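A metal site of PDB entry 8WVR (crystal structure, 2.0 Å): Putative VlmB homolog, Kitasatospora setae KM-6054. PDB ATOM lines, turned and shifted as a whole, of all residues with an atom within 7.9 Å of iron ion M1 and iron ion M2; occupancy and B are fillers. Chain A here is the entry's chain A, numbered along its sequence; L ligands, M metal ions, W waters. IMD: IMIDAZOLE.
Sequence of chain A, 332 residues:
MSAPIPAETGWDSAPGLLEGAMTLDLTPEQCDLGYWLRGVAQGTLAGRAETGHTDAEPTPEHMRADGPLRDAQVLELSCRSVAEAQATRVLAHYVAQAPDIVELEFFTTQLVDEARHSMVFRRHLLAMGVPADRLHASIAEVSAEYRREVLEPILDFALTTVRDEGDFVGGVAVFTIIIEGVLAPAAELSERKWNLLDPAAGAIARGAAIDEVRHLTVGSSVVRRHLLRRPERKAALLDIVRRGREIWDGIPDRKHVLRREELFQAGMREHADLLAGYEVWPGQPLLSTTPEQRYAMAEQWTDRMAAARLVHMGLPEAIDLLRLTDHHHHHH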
ATOM      1  N   ARG A  80      -5.834   6.941   3.788  1.00  0.00           N
ATOM      2  CA  ARG A  80      -5.511   8.363   3.847  1.00  0.00           C
ATOM      3  C   ARG A  80      -6.031   9.009   5.122  1.00  0.00           C
ATOM      4  O   ARG A  80      -5.353   9.840   5.739  1.00  0.00           O
ATOM      5  CB  ARG A  80      -6.066   9.082   2.622  1.00  0.00           C
ATOM      6  CG  ARG A  80      -5.316   8.797   1.323  1.00  0.00           C
ATOM      7  CD  ARG A  80      -5.777   9.718   0.221  1.00  0.00           C
ATOM      8  NE  ARG A  80      -5.130   9.375  -1.040  1.00  0.00           N
ATOM      9  CZ  ARG A  80      -3.870   9.654  -1.312  1.00  0.00           C
ATOM     10  NH1 ARG A  80      -3.094  10.292  -0.439  1.00  0.00           N
ATOM     11  NH2 ARG A  80      -3.351   9.280  -2.480  1.00  0.00           N
ATOM     12  N   ALA A  83      -3.745   8.082   7.891  1.00  0.00           N
ATOM     13  CA  ALA A  83      -2.431   8.708   7.712  1.00  0.00           C
ATOM     14  C   ALA A  83      -2.464  10.176   8.111  1.00  0.00           C
ATOM     15  O   ALA A  83      -1.549  10.665   8.786  1.00  0.00           O
ATOM     16  CB  ALA A  83      -1.986   8.549   6.244  1.00  0.00           C
ATOM     17  N   GLU A  84      -3.508  10.896   7.696  1.00  0.00           N
ATOM     18  CA  GLU A  84      -3.615  12.314   7.982  1.00  0.00           C
ATOM     19  C   GLU A  84      -3.866  12.566   9.465  1.00  0.00           C
ATOM     20  O   GLU A  84      -3.395  13.579  10.006  1.00  0.00           O
ATOM     21  CB  GLU A  84      -4.718  12.944   7.123  1.00  0.00           C
ATOM     22  CG  GLU A  84      -4.456  12.897   5.605  1.00  0.00           C
ATOM     23  CD  GLU A  84      -3.242  13.703   5.182  1.00  0.00           C
ATOM     24  OE1 GLU A  84      -2.118  13.434   5.682  1.00  0.00           O
ATOM     25  OE2 GLU A  84      -3.405  14.628   4.349  1.00  0.00           O
ATOM     26  N   ALA A  87      -0.533  12.021  11.119  1.00  0.00           N
ATOM     27  CA  ALA A  87       0.329  13.138  10.775  1.00  0.00           C
ATOM     28  C   ALA A  87       0.021  14.364  11.621  1.00  0.00           C
ATOM     29  O   ALA A  87       0.928  15.115  12.005  1.00  0.00           O
ATOM     30  CB  ALA A  87       0.189  13.469   9.279  1.00  0.00           C
ATOM     31  N   LEU A  91       2.720  16.299  13.713  1.00  0.00           N
ATOM     32  CA  LEU A  91       2.930  17.722  13.502  1.00  0.00           C
ATOM     33  C   LEU A  91       2.744  18.541  14.784  1.00  0.00           C
ATOM     34  O   LEU A  91       3.310  19.628  14.911  1.00  0.00           O
ATOM     35  CB  LEU A  91       1.967  18.220  12.420  1.00  0.00           C
ATOM     36  CG  LEU A  91       2.420  17.798  11.008  1.00  0.00           C
ATOM     37  CD1 LEU A  91       1.292  18.059  10.022  1.00  0.00           C
ATOM     38  CD2 LEU A  91       3.737  18.494  10.555  1.00  0.00           C
ATOM     39  N   GLN A 110      -0.579  24.079   9.123  1.00  0.00           N
ATOM     40  CA  GLN A 110      -0.446  22.789   8.462  1.00  0.00           C
ATOM     41  C   GLN A 110      -1.058  21.690   9.302  1.00  0.00           C
ATOM     42  O   GLN A 110      -1.702  20.774   8.768  1.00  0.00           O
ATOM     43  CB  GLN A 110       1.023  22.474   8.145  1.00  0.00           C
ATOM     44  CG  GLN A 110       1.152  21.053   7.589  1.00  0.00           C
ATOM     45  CD  GLN A 110       2.478  20.745   6.907  1.00  0.00           C
ATOM     46  OE1 GLN A 110       3.401  21.564   6.907  1.00  0.00           O
ATOM     47  NE2 GLN A 110       2.569  19.553   6.312  1.00  0.00           N
ATOM     48  N   ASP A 113      -4.622  21.829   8.604  1.00  0.00           N
ATOM     49  CA  ASP A 113      -4.837  21.310   7.249  1.00  0.00           C
ATOM     50  C   ASP A 113      -4.892  19.798   7.264  1.00  0.00           C
ATOM     51  O   ASP A 113      -5.802  19.194   6.677  1.00  0.00           O
ATOM     52  CB  ASP A 113      -3.702  21.779   6.301  1.00  0.00           C
ATOM     53  CG  ASP A 113      -3.835  23.225   5.883  1.00  0.00           C
ATOM     54  OD1 ASP A 113      -4.935  23.791   5.988  1.00  0.00           O
ATOM     55  OD2 ASP A 113      -2.813  23.801   5.417  1.00  0.00           O
ATOM     56  N   GLU A 114      -3.935  19.149   7.934  1.00  0.00           N
ATOM     57  CA  GLU A 114      -3.922  17.689   7.902  1.00  0.00           C
ATOM     58  C   GLU A 114      -5.101  17.104   8.663  1.00  0.00           C
ATOM     59  O   GLU A 114      -5.665  16.079   8.259  1.00  0.00           O
ATOM     60  CB  GLU A 114      -2.609  17.145   8.482  1.00  0.00           C
ATOM     61  CG  GLU A 114      -1.327  17.676   7.875  1.00  0.00           C
ATOM     62  CD  GLU A 114      -1.178  17.467   6.359  1.00  0.00           C
ATOM     63  OE1 GLU A 114      -1.972  16.752   5.744  1.00  0.00           O
ATOM     64  OE2 GLU A 114      -0.223  18.027   5.797  1.00  0.00           O
ATOM     65  N   ALA A 115      -5.485  17.738   9.768  1.00  0.00           N
ATOM     66  CA  ALA A 115      -6.676  17.284  10.466  1.00  0.00           C
ATOM     67  C   ALA A 115      -7.899  17.420   9.574  1.00  0.00           C
ATOM     68  O   ALA A 115      -8.782  16.547   9.577  1.00  0.00           O
ATOM     69  CB  ALA A 115      -6.866  18.058  11.766  1.00  0.00           C
ATOM     70  N   ARG A 116      -7.972  18.505   8.789  1.00  0.00           N
ATOM     71  CA  ARG A 116      -9.069  18.665   7.830  1.00  0.00           C
ATOM     72  C   ARG A 116      -9.042  17.567   6.765  1.00  0.00           C
ATOM     73  O   ARG A 116     -10.091  17.005   6.429  1.00  0.00           O
ATOM     74  CB  ARG A 116      -8.986  20.045   7.167  1.00  0.00           C
ATOM     75  CG  ARG A 116     -10.277  20.424   6.422  1.00  0.00           C
ATOM     76  CD  ARG A 116     -10.120  21.697   5.604  1.00  0.00           C
ATOM     77  NE  ARG A 116      -9.217  21.521   4.461  1.00  0.00           N
ATOM     78  CZ  ARG A 116      -9.518  20.819   3.382  1.00  0.00           C
ATOM     79  NH1 ARG A 116     -10.700  20.222   3.240  1.00  0.00           N
ATOM     80  NH2 ARG A 116      -8.613  20.717   2.397  1.00  0.00           N
ATOM     81  N   HIS A 117      -7.858  17.256   6.227  1.00  0.00           N
ATOM     82  CA  HIS A 117      -7.756  16.183   5.254  1.00  0.00           C
ATOM     83  C   HIS A 117      -8.277  14.882   5.828  1.00  0.00           C
ATOM     84  O   HIS A 117      -9.061  14.186   5.181  1.00  0.00           O
ATOM     85  CB  HIS A 117      -6.300  16.027   4.802  1.00  0.00           C
ATOM     86  CG  HIS A 117      -5.771  17.257   4.144  1.00  0.00           C
ATOM     87  ND1 HIS A 117      -4.449  17.442   3.831  1.00  0.00           N
ATOM     88  CD2 HIS A 117      -6.415  18.391   3.759  1.00  0.00           C
ATOM     89  CE1 HIS A 117      -4.295  18.627   3.269  1.00  0.00           C
ATOM     90  NE2 HIS A 117      -5.470  19.232   3.232  1.00  0.00           N
ATOM     91  N   SER A 118      -7.860  14.558   7.060  1.00  0.00           N
ATOM     92  CA  SER A 118      -8.373  13.354   7.696  1.00  0.00           C
ATOM     93  C   SER A 118      -9.891  13.397   7.756  1.00  0.00           C
ATOM     94  O   SER A 118     -10.556  12.380   7.531  1.00  0.00           O
ATOM     95  CB  SER A 118      -7.817  13.206   9.113  1.00  0.00           C
ATOM     96  OG  SER A 118      -8.221  11.974   9.684  1.00  0.00           O
ATOM     97  N   PHE A 121     -11.686  13.052   4.252  1.00  0.00           N
ATOM     98  CA  PHE A 121     -11.567  11.684   3.774  1.00  0.00           C
ATOM     99  C   PHE A 121     -12.520  10.755   4.519  1.00  0.00           C
ATOM    100  O   PHE A 121     -13.190   9.925   3.896  1.00  0.00           O
ATOM    101  CB  PHE A 121     -10.108  11.188   3.915  1.00  0.00           C
ATOM    102  CG  PHE A 121      -9.142  11.858   2.972  1.00  0.00           C
ATOM    103  CD1 PHE A 121      -9.554  12.269   1.720  1.00  0.00           C
ATOM    104  CD2 PHE A 121      -7.833  12.091   3.351  1.00  0.00           C
ATOM    105  CE1 PHE A 121      -8.671  12.904   0.843  1.00  0.00           C
ATOM    106  CE2 PHE A 121      -6.938  12.708   2.499  1.00  0.00           C
ATOM    107  CZ  PHE A 121      -7.357  13.121   1.240  1.00  0.00           C
ATOM    108  N   PHE A 175       9.698  15.400   7.227  1.00  0.00           N
ATOM    109  CA  PHE A 175       8.298  15.505   6.835  1.00  0.00           C
ATOM    110  C   PHE A 175       8.161  15.949   5.382  1.00  0.00           C
ATOM    111  O   PHE A 175       7.312  15.445   4.642  1.00  0.00           O
ATOM    112  CB  PHE A 175       7.548  16.453   7.771  1.00  0.00           C
ATOM    113  CG  PHE A 175       6.087  16.122   7.906  1.00  0.00           C
ATOM    114  CD1 PHE A 175       5.171  16.563   6.959  1.00  0.00           C
ATOM    115  CD2 PHE A 175       5.634  15.352   8.973  1.00  0.00           C
ATOM    116  CE1 PHE A 175       3.819  16.246   7.068  1.00  0.00           C
ATOM    117  CE2 PHE A 175       4.280  15.013   9.091  1.00  0.00           C
ATOM    118  CZ  PHE A 175       3.367  15.480   8.121  1.00  0.00           C
ATOM    119  N   GLU A 180       5.907  13.839   2.761  1.00  0.00           N
ATOM    120  CA  GLU A 180       5.009  14.488   1.803  1.00  0.00           C
ATOM    121  C   GLU A 180       5.629  14.531   0.412  1.00  0.00           C
ATOM    122  O   GLU A 180       4.936  14.338  -0.590  1.00  0.00           O
ATOM    123  CB  GLU A 180       4.649  15.883   2.286  1.00  0.00           C
ATOM    124  CG  GLU A 180       3.786  15.836   3.565  1.00  0.00           C
ATOM    125  CD  GLU A 180       2.987  17.092   3.801  1.00  0.00           C
ATOM    126  OE1 GLU A 180       3.583  18.195   3.780  1.00  0.00           O
ATOM    127  OE2 GLU A 180       1.764  16.949   4.022  1.00  0.00           O
ATOM    128  N   ALA A 184       2.974  12.978  -2.040  1.00  0.00           N
ATOM    129  CA  ALA A 184       2.104  13.923  -2.745  1.00  0.00           C
ATOM    130  C   ALA A 184       1.845  13.548  -4.212  1.00  0.00           C
ATOM    131  O   ALA A 184       0.726  13.808  -4.678  1.00  0.00           O
ATOM    132  CB  ALA A 184       2.679  15.333  -2.629  1.00  0.00           C
ATOM    133  N   ALA A 187      -1.112  11.607  -4.501  1.00  0.00           N
ATOM    134  CA  ALA A 187      -2.300  12.419  -4.258  1.00  0.00           C
ATOM    135  C   ALA A 187      -2.725  13.146  -5.531  1.00  0.00           C
ATOM    136  O   ALA A 187      -3.918  13.179  -5.870  1.00  0.00           O
ATOM    137  CB  ALA A 187      -2.060  13.408  -3.123  1.00  0.00           C
ATOM    138  N   ALA A 208      -7.292  19.549  -0.944  1.00  0.00           N
ATOM    139  CA  ALA A 208      -6.096  19.089  -0.233  1.00  0.00           C
ATOM    140  C   ALA A 208      -4.823  19.341  -1.037  1.00  0.00           C
ATOM    141  O   ALA A 208      -3.768  19.666  -0.468  1.00  0.00           O
ATOM    142  CB  ALA A 208      -6.245  17.604   0.128  1.00  0.00           C
ATOM    143  N   ALA A 209      -4.901  19.193  -2.368  1.00  0.00           N
ATOM    144  CA  ALA A 209      -3.720  19.416  -3.208  1.00  0.00           C
ATOM    145  C   ALA A 209      -3.309  20.880  -3.162  1.00  0.00           C
ATOM    146  O   ALA A 209      -2.114  21.192  -3.114  1.00  0.00           O
ATOM    147  CB  ALA A 209      -3.983  18.973  -4.649  1.00  0.00           C
ATOM    148  N   ASP A 211      -3.766  22.870  -0.585  1.00  0.00           N
ATOM    149  CA  ASP A 211      -3.058  22.918   0.695  1.00  0.00           C
ATOM    150  C   ASP A 211      -1.643  22.375   0.544  1.00  0.00           C
ATOM    151  O   ASP A 211      -0.686  22.970   1.044  1.00  0.00           O
ATOM    152  CB  ASP A 211      -3.811  22.096   1.759  1.00  0.00           C
ATOM    153  CG  ASP A 211      -5.200  22.635   2.080  1.00  0.00           C
ATOM    154  OD1 ASP A 211      -5.436  23.860   1.971  1.00  0.00           O
ATOM    155  OD2 ASP A 211      -6.051  21.816   2.472  1.00  0.00           O
ATOM    156  N   GLU A 212      -1.495  21.246  -0.141  1.00  0.00           N
ATOM    157  CA  GLU A 212      -0.212  20.560  -0.199  1.00  0.00           C
ATOM    158  C   GLU A 212       0.829  21.357  -0.966  1.00  0.00           C
ATOM    159  O   GLU A 212       2.021  21.299  -0.648  1.00  0.00           O
ATOM    160  CB  GLU A 212      -0.385  19.162  -0.806  1.00  0.00           C
ATOM    161  CG  GLU A 212       0.847  18.258  -0.740  1.00  0.00           C
ATOM    162  CD  GLU A 212       1.146  17.738   0.667  1.00  0.00           C
ATOM    163  OE1 GLU A 212       0.858  18.446   1.636  1.00  0.00           O
ATOM    164  OE2 GLU A 212       1.706  16.640   0.807  1.00  0.00           O
ATOM    165  N   VAL A 213       0.399  22.138  -1.969  1.00  0.00           N
ATOM    166  CA  VAL A 213       1.333  23.047  -2.633  1.00  0.00           C
ATOM    167  C   VAL A 213       2.012  23.922  -1.588  1.00  0.00           C
ATOM    168  O   VAL A 213       3.240  24.105  -1.608  1.00  0.00           O
ATOM    169  CB  VAL A 213       0.604  23.893  -3.691  1.00  0.00           C
ATOM    170  CG1 VAL A 213       1.503  25.024  -4.175  1.00  0.00           C
ATOM    171  CG2 VAL A 213       0.145  23.034  -4.864  1.00  0.00           C
ATOM    172  N   ARG A 214       1.214  24.450  -0.662  1.00  0.00           N
ATOM    173  CA  ARG A 214       1.735  25.292   0.409  1.00  0.00           C
ATOM    174  C   ARG A 214       2.612  24.487   1.370  1.00  0.00           C
ATOM    175  O   ARG A 214       3.697  24.936   1.738  1.00  0.00           O
ATOM    176  CB  ARG A 214       0.563  25.953   1.148  1.00  0.00           C
ATOM    177  CG  ARG A 214       0.950  26.824   2.364  1.00  0.00           C
ATOM    178  CD  ARG A 214      -0.284  27.529   2.979  1.00  0.00           C
ATOM    179  NE  ARG A 214      -1.334  26.602   3.411  1.00  0.00           N
ATOM    180  CZ  ARG A 214      -2.417  26.283   2.703  1.00  0.00           C
ATOM    181  NH1 ARG A 214      -2.642  26.802   1.491  1.00  0.00           N
ATOM    182  NH2 ARG A 214      -3.304  25.443   3.219  1.00  0.00           N
ATOM    183  N   HIS A 215       2.160  23.303   1.803  1.00  0.00           N
ATOM    184  CA  HIS A 215       2.990  22.503   2.711  1.00  0.00           C
ATOM    185  C   HIS A 215       4.357  22.227   2.098  1.00  0.00           C
ATOM    186  O   HIS A 215       5.392  22.384   2.761  1.00  0.00           O
ATOM    187  CB  HIS A 215       2.309  21.168   3.076  1.00  0.00           C
ATOM    188  CG  HIS A 215       0.956  21.315   3.708  1.00  0.00           C
ATOM    189  ND1 HIS A 215       0.122  20.233   3.953  1.00  0.00           N
ATOM    190  CD2 HIS A 215       0.288  22.409   4.152  1.00  0.00           C
ATOM    191  CE1 HIS A 215      -1.000  20.665   4.497  1.00  0.00           C
ATOM    192  NE2 HIS A 215      -0.919  21.980   4.637  1.00  0.00           N
ATOM    193  N   LEU A 216       4.370  21.813   0.828  1.00  0.00           N
ATOM    194  CA  LEU A 216       5.611  21.395   0.178  1.00  0.00           C
ATOM    195  C   LEU A 216       6.548  22.582  -0.047  1.00  0.00           C
ATOM    196  O   LEU A 216       7.749  22.484   0.224  1.00  0.00           O
ATOM    197  CB  LEU A 216       5.281  20.706  -1.147  1.00  0.00           C
ATOM    198  CG  LEU A 216       4.685  19.309  -0.990  1.00  0.00           C
ATOM    199  CD1 LEU A 216       4.188  18.789  -2.349  1.00  0.00           C
ATOM    200  CD2 LEU A 216       5.716  18.363  -0.378  1.00  0.00           C
HETATM  201  N1  IMD L   1      -3.027  15.592   1.630  1.00  0.00           N
HETATM  202  C2  IMD L   1      -3.772  14.561   1.155  1.00  0.00           C
HETATM  203  N3  IMD L   1      -3.908  14.731  -0.157  1.00  0.00           N
HETATM  204  C4  IMD L   1      -3.256  15.870  -0.523  1.00  0.00           C
HETATM  205  C5  IMD L   1      -2.710  16.398   0.600  1.00  0.00           C
HETATM  206 FE    FE M   1       0.291  18.142   3.665  1.00  0.00          FE
HETATM  207 FE    FE M   2      -2.603  16.293   3.733  1.00  0.00          FE
HETATM  208  O   HOH W   1      -1.558  17.665   3.101  1.00  0.00           O
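Gln 110 touches iron ion M1. Within 4 Å of iron ion M1: Gln 110, Glu 114, Glu 180, Glu 212 and His 215. The nearest printed residue that does not touch iron ion M1 is His 117 (4.6 Å).
The side-chain amide nitrogen of Gln 110 lies within hydrogen-bond range of the side-chain carboxylate of Glu 180 (3.0 Å). The backbone NH (N) of Glu 180 lies within hydrogen-bond range of the backbone carbonyl oxygen (O) of Phe 175, at 2.8 Å. NE2 of Gln 110 sits close to ND1 of His 215 (3.5 Å). A ring nitrogen (NE2) of His 215 lies within hydrogen-bond range of the side-chain carboxylate of Asp 113 (2.7 Å). OE2 of Glu 114 lies close to NE2 of Gln 110 (3.2 Å). NE2 of His 117 lies close to O of Asp 113 (3.5 Å). NE2 of His 117 lies within hydrogen-bond range of OD2 of Asp 211.
Iron ion M2 is bound by water W1 (1.8 Å). OE2 of Glu 84 binds iron ion M2. OE1 of Glu 114 binds iron ion M2, 2.2 Å away. ND1 of His 117 is bound to iron ion M2 (2.2 Å). Iron ion M2 is bound by a nitrogen (N1) of the ligand, at 2.3 Å. Iron ion M2 has five donor atoms within binding distance.
Along chain A the residues within 4 Å of iron ion M2 span positions 84 to 117.
Iron ion M1 is bound by the side-chain carboxylate of Glu 180, water W1, a ring nitrogen (ND1) of His 215, the side-chain carboxylate of Glu 212 and the side-chain carboxylate of Glu 114. Iron ion M1 has five donor atoms within binding distance.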
